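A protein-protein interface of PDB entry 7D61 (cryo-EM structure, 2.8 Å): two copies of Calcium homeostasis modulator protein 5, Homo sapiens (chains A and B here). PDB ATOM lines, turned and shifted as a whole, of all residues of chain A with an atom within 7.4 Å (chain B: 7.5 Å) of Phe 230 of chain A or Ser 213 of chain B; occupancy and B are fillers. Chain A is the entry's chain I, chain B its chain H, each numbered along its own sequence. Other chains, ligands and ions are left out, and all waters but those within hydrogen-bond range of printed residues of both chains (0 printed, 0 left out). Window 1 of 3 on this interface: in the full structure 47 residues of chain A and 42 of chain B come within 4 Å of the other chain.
The side-chain amino group (NZ) of Lys 221 of chain B sits close to the backbone carbonyl oxygen (O) of Leu 231 of chain A (3.5 Å).
The side-chain amide nitrogen (ND2) of Asn 235 of chain A sits close to the side-chain amino group (NZ) of Lys 221 of chain B (3.1 Å).
Of chain B, only Leu 210 (3.7 Å), Ser 213 (3.9 Å) and Phe 214 (3.8 Å) come within 4 Å of Phe 230 of chain A.
Of chain A, only Phe 230 (3.9 Å) comes within 4 Å of Ser 213 of chain B.
Of the printed residues of chain B, Leu 231 of chain A touches Lys 221 (3.4 Å).
Printed residues of chain B within 4 Å of Leu 226 of chain A: Leu 210 (3.7 Å).
Of the printed residues of chain B, Met 256 of chain A touches Phe 214 (3.7 Å).
Of the printed residues of chain B, Trp 262 of chain A touches Leu 210 and Gln 211.
Val 207 of chain B touches none of the printed residues of chain A.
Gln 225 of chain A touches none of the printed residues of chain B.
The nearest residue of chain B that does not touch Phe 230 of chain A is Thr 217 of chain B (4.2 Å).
The nearest residue of chain A that does not touch Ser 213 of chain B is Leu 226 of chain A (6.1 Å).
Hydrophobic or aromatic side chains of chain A within 4 Å of the printed part of chain B: Leu 226, Phe 230, Leu 231, Ala 234, Met 256 and Trp 262.
Of the 13 printed residues of chain B, 5 touch a printed residue of chain A.
Printed residues of chain B that touch a printed residue of chain A: Leu 210, Gln 211, Ser 213, Phe 214 and Lys 221.
Hydrophobic or aromatic side chains of chain B that line the printed part of chain A: Leu 210 and Phe 214.
Along chain B the printed residues that touch a printed residue of chain A span positions 210 to 221.
Among the printed residues, 10 pairs touch across the chains.
Among the printed residues, no Asp or Glu carboxylate lies within 4 Å of a Lys or Arg side-chain nitrogen of the other chain.
No position is printed for both chains.
Leu 210 of chain B touches Leu 226 of chain A (CD1 to CD2, 3.7 Å).
O of Leu 210 of chain B touches CZ of Phe 230 of chain A, at 3.7 Å.
Phe 230 of chain A touches Ser 213 of chain B (CE2 to OG, 3.9 Å).
Phe 214 of chain B touches Phe 230 of chain A (CD1 to CD1, 3.8 Å).
CB of Ala 234 of chain A touches CD of Lys 221 of chain B, 3.8 Å away.
Met 256 of chain A touches Phe 214 of chain B (CE to CE2, 3.7 Å).
Trp 262 of chain A touches Leu 210 of chain B (CZ3 to O, 3.7 Å).
Trp 262 of chain A touches Gln 211 of chain B (CD1 to NE2, 3.7 Å).
The backbone carbonyl oxygen (O) of Ser 213 of chain B lies within hydrogen-bond range of the side-chain hydroxyl (OG1) of Thr 217 of chain B (2.6 Å).
The backbone carbonyl oxygen (O) of Leu 231 of chain A sits at hydrogen-bond distance from the side-chain amide nitrogen (ND2) of Asn 235 of chain A (3.5 Å).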
ATOM      1  N   GLN A 225      30.495  -7.239  18.479  1.00  0.00           N
ATOM      2  CA  GLN A 225      30.374  -6.017  17.693  1.00  0.00           C
ATOM      3  C   GLN A 225      29.419  -5.027  18.344  1.00  0.00           C
ATOM      4  O   GLN A 225      29.477  -3.829  18.051  1.00  0.00           O
ATOM      5  CB  GLN A 225      29.911  -6.348  16.276  1.00  0.00           C
ATOM      6  CG  GLN A 225      30.919  -7.124  15.450  1.00  0.00           C
ATOM      7  CD  GLN A 225      32.029  -6.250  14.914  1.00  0.00           C
ATOM      8  OE1 GLN A 225      33.188  -6.388  15.303  1.00  0.00           O
ATOM      9  NE2 GLN A 225      31.679  -5.336  14.017  1.00  0.00           N
ATOM     10  N   LEU A 226      28.534  -5.505  19.220  1.00  0.00           N
ATOM     11  CA  LEU A 226      27.651  -4.606  19.953  1.00  0.00           C
ATOM     12  C   LEU A 226      28.401  -3.855  21.044  1.00  0.00           C
ATOM     13  O   LEU A 226      28.072  -2.703  21.340  1.00  0.00           O
ATOM     14  CB  LEU A 226      26.493  -5.392  20.559  1.00  0.00           C
ATOM     15  CG  LEU A 226      25.201  -4.650  20.875  1.00  0.00           C
ATOM     16  CD1 LEU A 226      24.619  -4.047  19.619  1.00  0.00           C
ATOM     17  CD2 LEU A 226      24.221  -5.608  21.510  1.00  0.00           C
ATOM     18  N   GLU A 227      29.406  -4.490  21.651  1.00  0.00           N
ATOM     19  CA  GLU A 227      30.200  -3.830  22.678  1.00  0.00           C
ATOM     20  C   GLU A 227      31.160  -2.801  22.100  1.00  0.00           C
ATOM     21  O   GLU A 227      31.638  -1.939  22.841  1.00  0.00           O
ATOM     22  CB  GLU A 227      30.986  -4.862  23.486  1.00  0.00           C
ATOM     23  CG  GLU A 227      30.127  -5.770  24.348  1.00  0.00           C
ATOM     24  CD  GLU A 227      30.890  -6.980  24.856  1.00  0.00           C
ATOM     25  OE1 GLU A 227      32.123  -7.028  24.664  1.00  0.00           O
ATOM     26  OE2 GLU A 227      30.259  -7.882  25.446  1.00  0.00           O
ATOM     27  N   ASN A 228      31.459  -2.874  20.805  1.00  0.00           N
ATOM     28  CA  ASN A 228      32.327  -1.894  20.170  1.00  0.00           C
ATOM     29  C   ASN A 228      31.559  -0.772  19.489  1.00  0.00           C
ATOM     30  O   ASN A 228      32.127   0.302  19.271  1.00  0.00           O
ATOM     31  CB  ASN A 228      33.237  -2.573  19.146  1.00  0.00           C
ATOM     32  CG  ASN A 228      34.160  -3.593  19.774  1.00  0.00           C
ATOM     33  OD1 ASN A 228      34.243  -3.698  20.996  1.00  0.00           O
ATOM     34  ND2 ASN A 228      34.861  -4.349  18.941  1.00  0.00           N
ATOM     35  N   THR A 229      30.290  -0.991  19.145  1.00  0.00           N
ATOM     36  CA  THR A 229      29.467   0.090  18.619  1.00  0.00           C
ATOM     37  C   THR A 229      28.908   0.957  19.740  1.00  0.00           C
ATOM     38  O   THR A 229      28.752   2.170  19.563  1.00  0.00           O
ATOM     39  CB  THR A 229      28.332  -0.482  17.767  1.00  0.00           C
ATOM     40  OG1 THR A 229      28.849  -1.521  16.930  1.00  0.00           O
ATOM     41  CG2 THR A 229      27.722   0.589  16.882  1.00  0.00           C
ATOM     42  N   PHE A 230      28.611   0.355  20.895  1.00  0.00           N
ATOM     43  CA  PHE A 230      28.184   1.131  22.054  1.00  0.00           C
ATOM     44  C   PHE A 230      29.327   1.974  22.601  1.00  0.00           C
ATOM     45  O   PHE A 230      29.126   3.134  22.973  1.00  0.00           O
ATOM     46  CB  PHE A 230      27.654   0.201  23.145  1.00  0.00           C
ATOM     47  CG  PHE A 230      26.246  -0.270  22.926  1.00  0.00           C
ATOM     48  CD1 PHE A 230      25.448   0.290  21.944  1.00  0.00           C
ATOM     49  CD2 PHE A 230      25.723  -1.282  23.710  1.00  0.00           C
ATOM     50  CE1 PHE A 230      24.153  -0.148  21.757  1.00  0.00           C
ATOM     51  CE2 PHE A 230      24.431  -1.727  23.523  1.00  0.00           C
ATOM     52  CZ  PHE A 230      23.646  -1.158  22.544  1.00  0.00           C
ATOM     53  N   LEU A 231      30.532   1.411  22.648  1.00  0.00           N
ATOM     54  CA  LEU A 231      31.681   2.104  23.213  1.00  0.00           C
ATOM     55  C   LEU A 231      32.206   3.203  22.300  1.00  0.00           C
ATOM     56  O   LEU A 231      32.864   4.129  22.783  1.00  0.00           O
ATOM     57  CB  LEU A 231      32.778   1.078  23.524  1.00  0.00           C
ATOM     58  CG  LEU A 231      34.028   1.398  24.344  1.00  0.00           C
ATOM     59  CD1 LEU A 231      34.407   0.176  25.153  1.00  0.00           C
ATOM     60  CD2 LEU A 231      35.194   1.795  23.453  1.00  0.00           C
ATOM     61  N   ASP A 232      31.920   3.131  21.003  1.00  0.00           N
ATOM     62  CA  ASP A 232      32.342   4.159  20.062  1.00  0.00           C
ATOM     63  C   ASP A 232      31.336   5.300  19.980  1.00  0.00           C
ATOM     64  O   ASP A 232      31.726   6.461  19.826  1.00  0.00           O
ATOM     65  CB  ASP A 232      32.560   3.535  18.680  1.00  0.00           C
ATOM     66  CG  ASP A 232      32.746   4.566  17.589  1.00  0.00           C
ATOM     67  OD1 ASP A 232      33.647   5.420  17.723  1.00  0.00           O
ATOM     68  OD2 ASP A 232      31.995   4.518  16.594  1.00  0.00           O
ATOM     69  N   TYR A 233      30.045   4.993  20.100  1.00  0.00           N
ATOM     70  CA  TYR A 233      29.020   6.027  20.098  1.00  0.00           C
ATOM     71  C   TYR A 233      28.910   6.750  21.432  1.00  0.00           C
ATOM     72  O   TYR A 233      28.327   7.836  21.484  1.00  0.00           O
ATOM     73  CB  TYR A 233      27.665   5.422  19.732  1.00  0.00           C
ATOM     74  CG  TYR A 233      27.341   5.500  18.260  1.00  0.00           C
ATOM     75  CD1 TYR A 233      26.369   6.373  17.790  1.00  0.00           C
ATOM     76  CD2 TYR A 233      28.008   4.704  17.340  1.00  0.00           C
ATOM     77  CE1 TYR A 233      26.068   6.450  16.445  1.00  0.00           C
ATOM     78  CE2 TYR A 233      27.715   4.772  15.991  1.00  0.00           C
ATOM     79  CZ  TYR A 233      26.744   5.648  15.551  1.00  0.00           C
ATOM     80  OH  TYR A 233      26.447   5.722  14.210  1.00  0.00           O
ATOM     81  N   ALA A 234      29.446   6.173  22.506  1.00  0.00           N
ATOM     82  CA  ALA A 234      29.456   6.834  23.804  1.00  0.00           C
ATOM     83  C   ALA A 234      30.648   7.757  23.986  1.00  0.00           C
ATOM     84  O   ALA A 234      30.582   8.672  24.814  1.00  0.00           O
ATOM     85  CB  ALA A 234      29.442   5.798  24.929  1.00  0.00           C
ATOM     86  N   ASN A 235      31.733   7.539  23.242  1.00  0.00           N
ATOM     87  CA  ASN A 235      32.853   8.468  23.256  1.00  0.00           C
ATOM     88  C   ASN A 235      32.578   9.713  22.430  1.00  0.00           C
ATOM     89  O   ASN A 235      33.194  10.754  22.677  1.00  0.00           O
ATOM     90  CB  ASN A 235      34.119   7.786  22.736  1.00  0.00           C
ATOM     91  CG  ASN A 235      34.964   7.204  23.845  1.00  0.00           C
ATOM     92  OD1 ASN A 235      35.041   7.758  24.939  1.00  0.00           O
ATOM     93  ND2 ASN A 235      35.617   6.084  23.564  1.00  0.00           N
ATOM     94  N   LYS A 236      31.674   9.628  21.459  1.00  0.00           N
ATOM     95  CA  LYS A 236      31.310  10.774  20.642  1.00  0.00           C
ATOM     96  C   LYS A 236      30.162  11.576  21.229  1.00  0.00           C
ATOM     97  O   LYS A 236      30.006  12.751  20.883  1.00  0.00           O
ATOM     98  CB  LYS A 236      30.934  10.319  19.230  1.00  0.00           C
ATOM     99  CG  LYS A 236      32.107   9.825  18.404  1.00  0.00           C
ATOM    100  CD  LYS A 236      31.633   9.075  17.173  1.00  0.00           C
ATOM    101  CE  LYS A 236      30.806   9.968  16.266  1.00  0.00           C
ATOM    102  NZ  LYS A 236      29.754   9.202  15.542  1.00  0.00           N
ATOM    103  N   MET A 256      20.341   9.217  16.554  1.00  0.00           N
ATOM    104  CA  MET A 256      20.248   8.028  17.382  1.00  0.00           C
ATOM    105  C   MET A 256      18.953   7.309  17.038  1.00  0.00           C
ATOM    106  O   MET A 256      18.026   7.932  16.507  1.00  0.00           O
ATOM    107  CB  MET A 256      20.271   8.381  18.879  1.00  0.00           C
ATOM    108  CG  MET A 256      21.653   8.688  19.428  1.00  0.00           C
ATOM    109  SD  MET A 256      22.716   7.235  19.496  1.00  0.00           S
ATOM    110  CE  MET A 256      22.056   6.405  20.936  1.00  0.00           C
ATOM    111  N   PRO A 257      18.872   5.998  17.285  1.00  0.00           N
ATOM    112  CA  PRO A 257      17.604   5.291  17.074  1.00  0.00           C
ATOM    113  C   PRO A 257      16.520   5.766  18.027  1.00  0.00           C
ATOM    114  O   PRO A 257      16.786   6.187  19.153  1.00  0.00           O
ATOM    115  CB  PRO A 257      17.962   3.821  17.335  1.00  0.00           C
ATOM    116  CG  PRO A 257      19.330   3.830  17.921  1.00  0.00           C
ATOM    117  CD  PRO A 257      19.995   5.058  17.429  1.00  0.00           C
ATOM    118  N   TRP A 262      14.245   0.895  19.562  1.00  0.00           N
ATOM    119  CA  TRP A 262      14.970   0.274  20.666  1.00  0.00           C
ATOM    120  C   TRP A 262      14.192  -0.898  21.251  1.00  0.00           C
ATOM    121  O   TRP A 262      14.777  -1.935  21.579  1.00  0.00           O
ATOM    122  CB  TRP A 262      15.261   1.307  21.756  1.00  0.00           C
ATOM    123  CG  TRP A 262      16.550   2.072  21.608  1.00  0.00           C
ATOM    124  CD1 TRP A 262      16.682   3.419  21.455  1.00  0.00           C
ATOM    125  CD2 TRP A 262      17.883   1.543  21.640  1.00  0.00           C
ATOM    126  NE1 TRP A 262      18.006   3.761  21.372  1.00  0.00           N
ATOM    127  CE2 TRP A 262      18.765   2.629  21.484  1.00  0.00           C
ATOM    128  CE3 TRP A 262      18.416   0.259  21.778  1.00  0.00           C
ATOM    129  CZ2 TRP A 262      20.147   2.470  21.461  1.00  0.00           C
ATOM    130  CZ3 TRP A 262      19.787   0.105  21.754  1.00  0.00           C
ATOM    131  CH2 TRP A 262      20.636   1.204  21.599  1.00  0.00           C
ATOM    132  N   VAL B 207      13.128   1.306  30.199  1.00  0.00           N
ATOM    133  CA  VAL B 207      13.738   0.903  28.944  1.00  0.00           C
ATOM    134  C   VAL B 207      13.890  -0.615  28.933  1.00  0.00           C
ATOM    135  O   VAL B 207      13.745  -1.286  29.954  1.00  0.00           O
ATOM    136  CB  VAL B 207      15.092   1.599  28.714  1.00  0.00           C
ATOM    137  CG1 VAL B 207      14.918   3.100  28.732  1.00  0.00           C
ATOM    138  CG2 VAL B 207      16.087   1.174  29.770  1.00  0.00           C
ATOM    139  N   SER B 208      14.187  -1.154  27.757  1.00  0.00           N
ATOM    140  CA  SER B 208      14.414  -2.581  27.600  1.00  0.00           C
ATOM    141  C   SER B 208      15.885  -2.893  27.868  1.00  0.00           C
ATOM    142  O   SER B 208      16.645  -2.044  28.335  1.00  0.00           O
ATOM    143  CB  SER B 208      13.976  -3.036  26.212  1.00  0.00           C
ATOM    144  OG  SER B 208      12.572  -3.208  26.153  1.00  0.00           O
ATOM    145  N   TYR B 209      16.301  -4.123  27.566  1.00  0.00           N
ATOM    146  CA  TYR B 209      17.643  -4.565  27.925  1.00  0.00           C
ATOM    147  C   TYR B 209      18.710  -3.947  27.032  1.00  0.00           C
ATOM    148  O   TYR B 209      19.846  -3.746  27.476  1.00  0.00           O
ATOM    149  CB  TYR B 209      17.723  -6.090  27.865  1.00  0.00           C
ATOM    150  CG  TYR B 209      19.088  -6.640  28.198  1.00  0.00           C
ATOM    151  CD1 TYR B 209      19.556  -6.635  29.507  1.00  0.00           C
ATOM    152  CD2 TYR B 209      19.919  -7.141  27.204  1.00  0.00           C
ATOM    153  CE1 TYR B 209      20.808  -7.129  29.819  1.00  0.00           C
ATOM    154  CE2 TYR B 209      21.174  -7.634  27.505  1.00  0.00           C
ATOM    155  CZ  TYR B 209      21.611  -7.626  28.815  1.00  0.00           C
ATOM    156  OH  TYR B 209      22.857  -8.117  29.120  1.00  0.00           O
ATOM    157  N   LEU B 210      18.370  -3.625  25.785  1.00  0.00           N
ATOM    158  CA  LEU B 210      19.374  -3.129  24.853  1.00  0.00           C
ATOM    159  C   LEU B 210      19.679  -1.654  25.086  1.00  0.00           C
ATOM    160  O   LEU B 210      20.839  -1.241  25.008  1.00  0.00           O
ATOM    161  CB  LEU B 210      18.908  -3.361  23.416  1.00  0.00           C
ATOM    162  CG  LEU B 210      19.970  -3.741  22.386  1.00  0.00           C
ATOM    163  CD1 LEU B 210      20.819  -4.886  22.897  1.00  0.00           C
ATOM    164  CD2 LEU B 210      19.313  -4.108  21.070  1.00  0.00           C
ATOM    165  N   GLN B 211      18.652  -0.853  25.377  1.00  0.00           N
ATOM    166  CA  GLN B 211      18.868   0.556  25.684  1.00  0.00           C
ATOM    167  C   GLN B 211      19.531   0.741  27.044  1.00  0.00           C
ATOM    168  O   GLN B 211      20.269   1.710  27.247  1.00  0.00           O
ATOM    169  CB  GLN B 211      17.537   1.305  25.624  1.00  0.00           C
ATOM    170  CG  GLN B 211      17.657   2.811  25.586  1.00  0.00           C
ATOM    171  CD  GLN B 211      16.354   3.481  25.228  1.00  0.00           C
ATOM    172  OE1 GLN B 211      15.299   2.852  25.239  1.00  0.00           O
ATOM    173  NE2 GLN B 211      16.417   4.764  24.905  1.00  0.00           N
ATOM    174  N   LEU B 212      19.290  -0.181  27.980  1.00  0.00           N
ATOM    175  CA  LEU B 212      19.919  -0.110  29.293  1.00  0.00           C
ATOM    176  C   LEU B 212      21.397  -0.473  29.243  1.00  0.00           C
ATOM    177  O   LEU B 212      22.151  -0.084  30.139  1.00  0.00           O
ATOM    178  CB  LEU B 212      19.176  -1.029  30.266  1.00  0.00           C
ATOM    179  CG  LEU B 212      19.434  -0.933  31.768  1.00  0.00           C
ATOM    180  CD1 LEU B 212      18.617   0.183  32.376  1.00  0.00           C
ATOM    181  CD2 LEU B 212      19.110  -2.252  32.436  1.00  0.00           C
ATOM    182  N   SER B 213      21.831  -1.195  28.211  1.00  0.00           N
ATOM    183  CA  SER B 213      23.241  -1.518  28.063  1.00  0.00           C
ATOM    184  C   SER B 213      24.035  -0.376  27.447  1.00  0.00           C
ATOM    185  O   SER B 213      25.253  -0.313  27.637  1.00  0.00           O
ATOM    186  CB  SER B 213      23.401  -2.781  27.218  1.00  0.00           C
ATOM    187  OG  SER B 213      24.760  -3.159  27.121  1.00  0.00           O
ATOM    188  N   PHE B 214      23.374   0.519  26.710  1.00  0.00           N
ATOM    189  CA  PHE B 214      24.020   1.737  26.238  1.00  0.00           C
ATOM    190  C   PHE B 214      24.035   2.809  27.319  1.00  0.00           C
ATOM    191  O   PHE B 214      24.975   3.609  27.380  1.00  0.00           O
ATOM    192  CB  PHE B 214      23.312   2.254  24.983  1.00  0.00           C
ATOM    193  CG  PHE B 214      23.869   3.547  24.457  1.00  0.00           C
ATOM    194  CD1 PHE B 214      25.076   3.570  23.780  1.00  0.00           C
ATOM    195  CD2 PHE B 214      23.184   4.739  24.639  1.00  0.00           C
ATOM    196  CE1 PHE B 214      25.592   4.757  23.299  1.00  0.00           C
ATOM    197  CE2 PHE B 214      23.697   5.926  24.164  1.00  0.00           C
ATOM    198  CZ  PHE B 214      24.901   5.934  23.492  1.00  0.00           C
ATOM    199  N   TRP B 215      23.004   2.834  28.167  1.00  0.00           N
ATOM    200  CA  TRP B 215      22.928   3.789  29.268  1.00  0.00           C
ATOM    201  C   TRP B 215      24.046   3.555  30.280  1.00  0.00           C
ATOM    202  O   TRP B 215      24.608   4.508  30.827  1.00  0.00           O
ATOM    203  CB  TRP B 215      21.553   3.670  29.928  1.00  0.00           C
ATOM    204  CG  TRP B 215      21.136   4.765  30.873  1.00  0.00           C
ATOM    205  CD1 TRP B 215      21.871   5.836  31.288  1.00  0.00           C
ATOM    206  CD2 TRP B 215      19.868   4.876  31.529  1.00  0.00           C
ATOM    207  NE1 TRP B 215      21.141   6.605  32.157  1.00  0.00           N
ATOM    208  CE2 TRP B 215      19.906   6.037  32.321  1.00  0.00           C
ATOM    209  CE3 TRP B 215      18.702   4.106  31.519  1.00  0.00           C
ATOM    210  CZ2 TRP B 215      18.824   6.446  33.096  1.00  0.00           C
ATOM    211  CZ3 TRP B 215      17.631   4.512  32.289  1.00  0.00           C
ATOM    212  CH2 TRP B 215      17.699   5.671  33.067  1.00  0.00           C
ATOM    213  N   LYS B 216      24.400   2.293  30.521  1.00  0.00           N
ATOM    214  CA  LYS B 216      25.473   1.992  31.458  1.00  0.00           C
ATOM    215  C   LYS B 216      26.849   2.242  30.856  1.00  0.00           C
ATOM    216  O   LYS B 216      27.805   2.496  31.594  1.00  0.00           O
ATOM    217  CB  LYS B 216      25.366   0.543  31.931  1.00  0.00           C
ATOM    218  CG  LYS B 216      24.266   0.306  32.946  1.00  0.00           C
ATOM    219  CD  LYS B 216      24.227  -1.147  33.381  1.00  0.00           C
ATOM    220  CE  LYS B 216      22.934  -1.472  34.105  1.00  0.00           C
ATOM    221  NZ  LYS B 216      22.421  -0.306  34.873  1.00  0.00           N
ATOM    222  N   THR B 217      26.971   2.167  29.531  1.00  0.00           N
ATOM    223  CA  THR B 217      28.244   2.458  28.882  1.00  0.00           C
ATOM    224  C   THR B 217      28.498   3.958  28.809  1.00  0.00           C
ATOM    225  O   THR B 217      29.640   4.406  28.954  1.00  0.00           O
ATOM    226  CB  THR B 217      28.272   1.846  27.481  1.00  0.00           C
ATOM    227  OG1 THR B 217      27.730   0.522  27.529  1.00  0.00           O
ATOM    228  CG2 THR B 217      29.693   1.779  26.947  1.00  0.00           C
ATOM    229  N   TYR B 218      27.444   4.746  28.589  1.00  0.00           N
ATOM    230  CA  TYR B 218      27.598   6.194  28.513  1.00  0.00           C
ATOM    231  C   TYR B 218      27.888   6.794  29.882  1.00  0.00           C
ATOM    232  O   TYR B 218      28.710   7.708  30.000  1.00  0.00           O
ATOM    233  CB  TYR B 218      26.346   6.825  27.909  1.00  0.00           C
ATOM    234  CG  TYR B 218      26.352   8.331  27.968  1.00  0.00           C
ATOM    235  CD1 TYR B 218      27.236   9.068  27.197  1.00  0.00           C
ATOM    236  CD2 TYR B 218      25.482   9.017  28.805  1.00  0.00           C
ATOM    237  CE1 TYR B 218      27.251  10.447  27.251  1.00  0.00           C
ATOM    238  CE2 TYR B 218      25.490  10.396  28.865  1.00  0.00           C
ATOM    239  CZ  TYR B 218      26.376  11.103  28.086  1.00  0.00           C
ATOM    240  OH  TYR B 218      26.390  12.476  28.141  1.00  0.00           O
ATOM    241  N   LYS B 221      31.777   6.301  31.004  1.00  0.00           N
ATOM    242  CA  LYS B 221      32.817   7.121  30.399  1.00  0.00           C
ATOM    243  C   LYS B 221      32.406   8.576  30.237  1.00  0.00           C
ATOM    244  O   LYS B 221      33.140   9.349  29.616  1.00  0.00           O
ATOM    245  CB  LYS B 221      33.243   6.546  29.052  1.00  0.00           C
ATOM    246  CG  LYS B 221      32.154   6.478  28.008  1.00  0.00           C
ATOM    247  CD  LYS B 221      32.744   5.982  26.705  1.00  0.00           C
ATOM    248  CE  LYS B 221      33.420   4.634  26.894  1.00  0.00           C
ATOM    249  NZ  LYS B 221      34.466   4.397  25.870  1.00  0.00           N
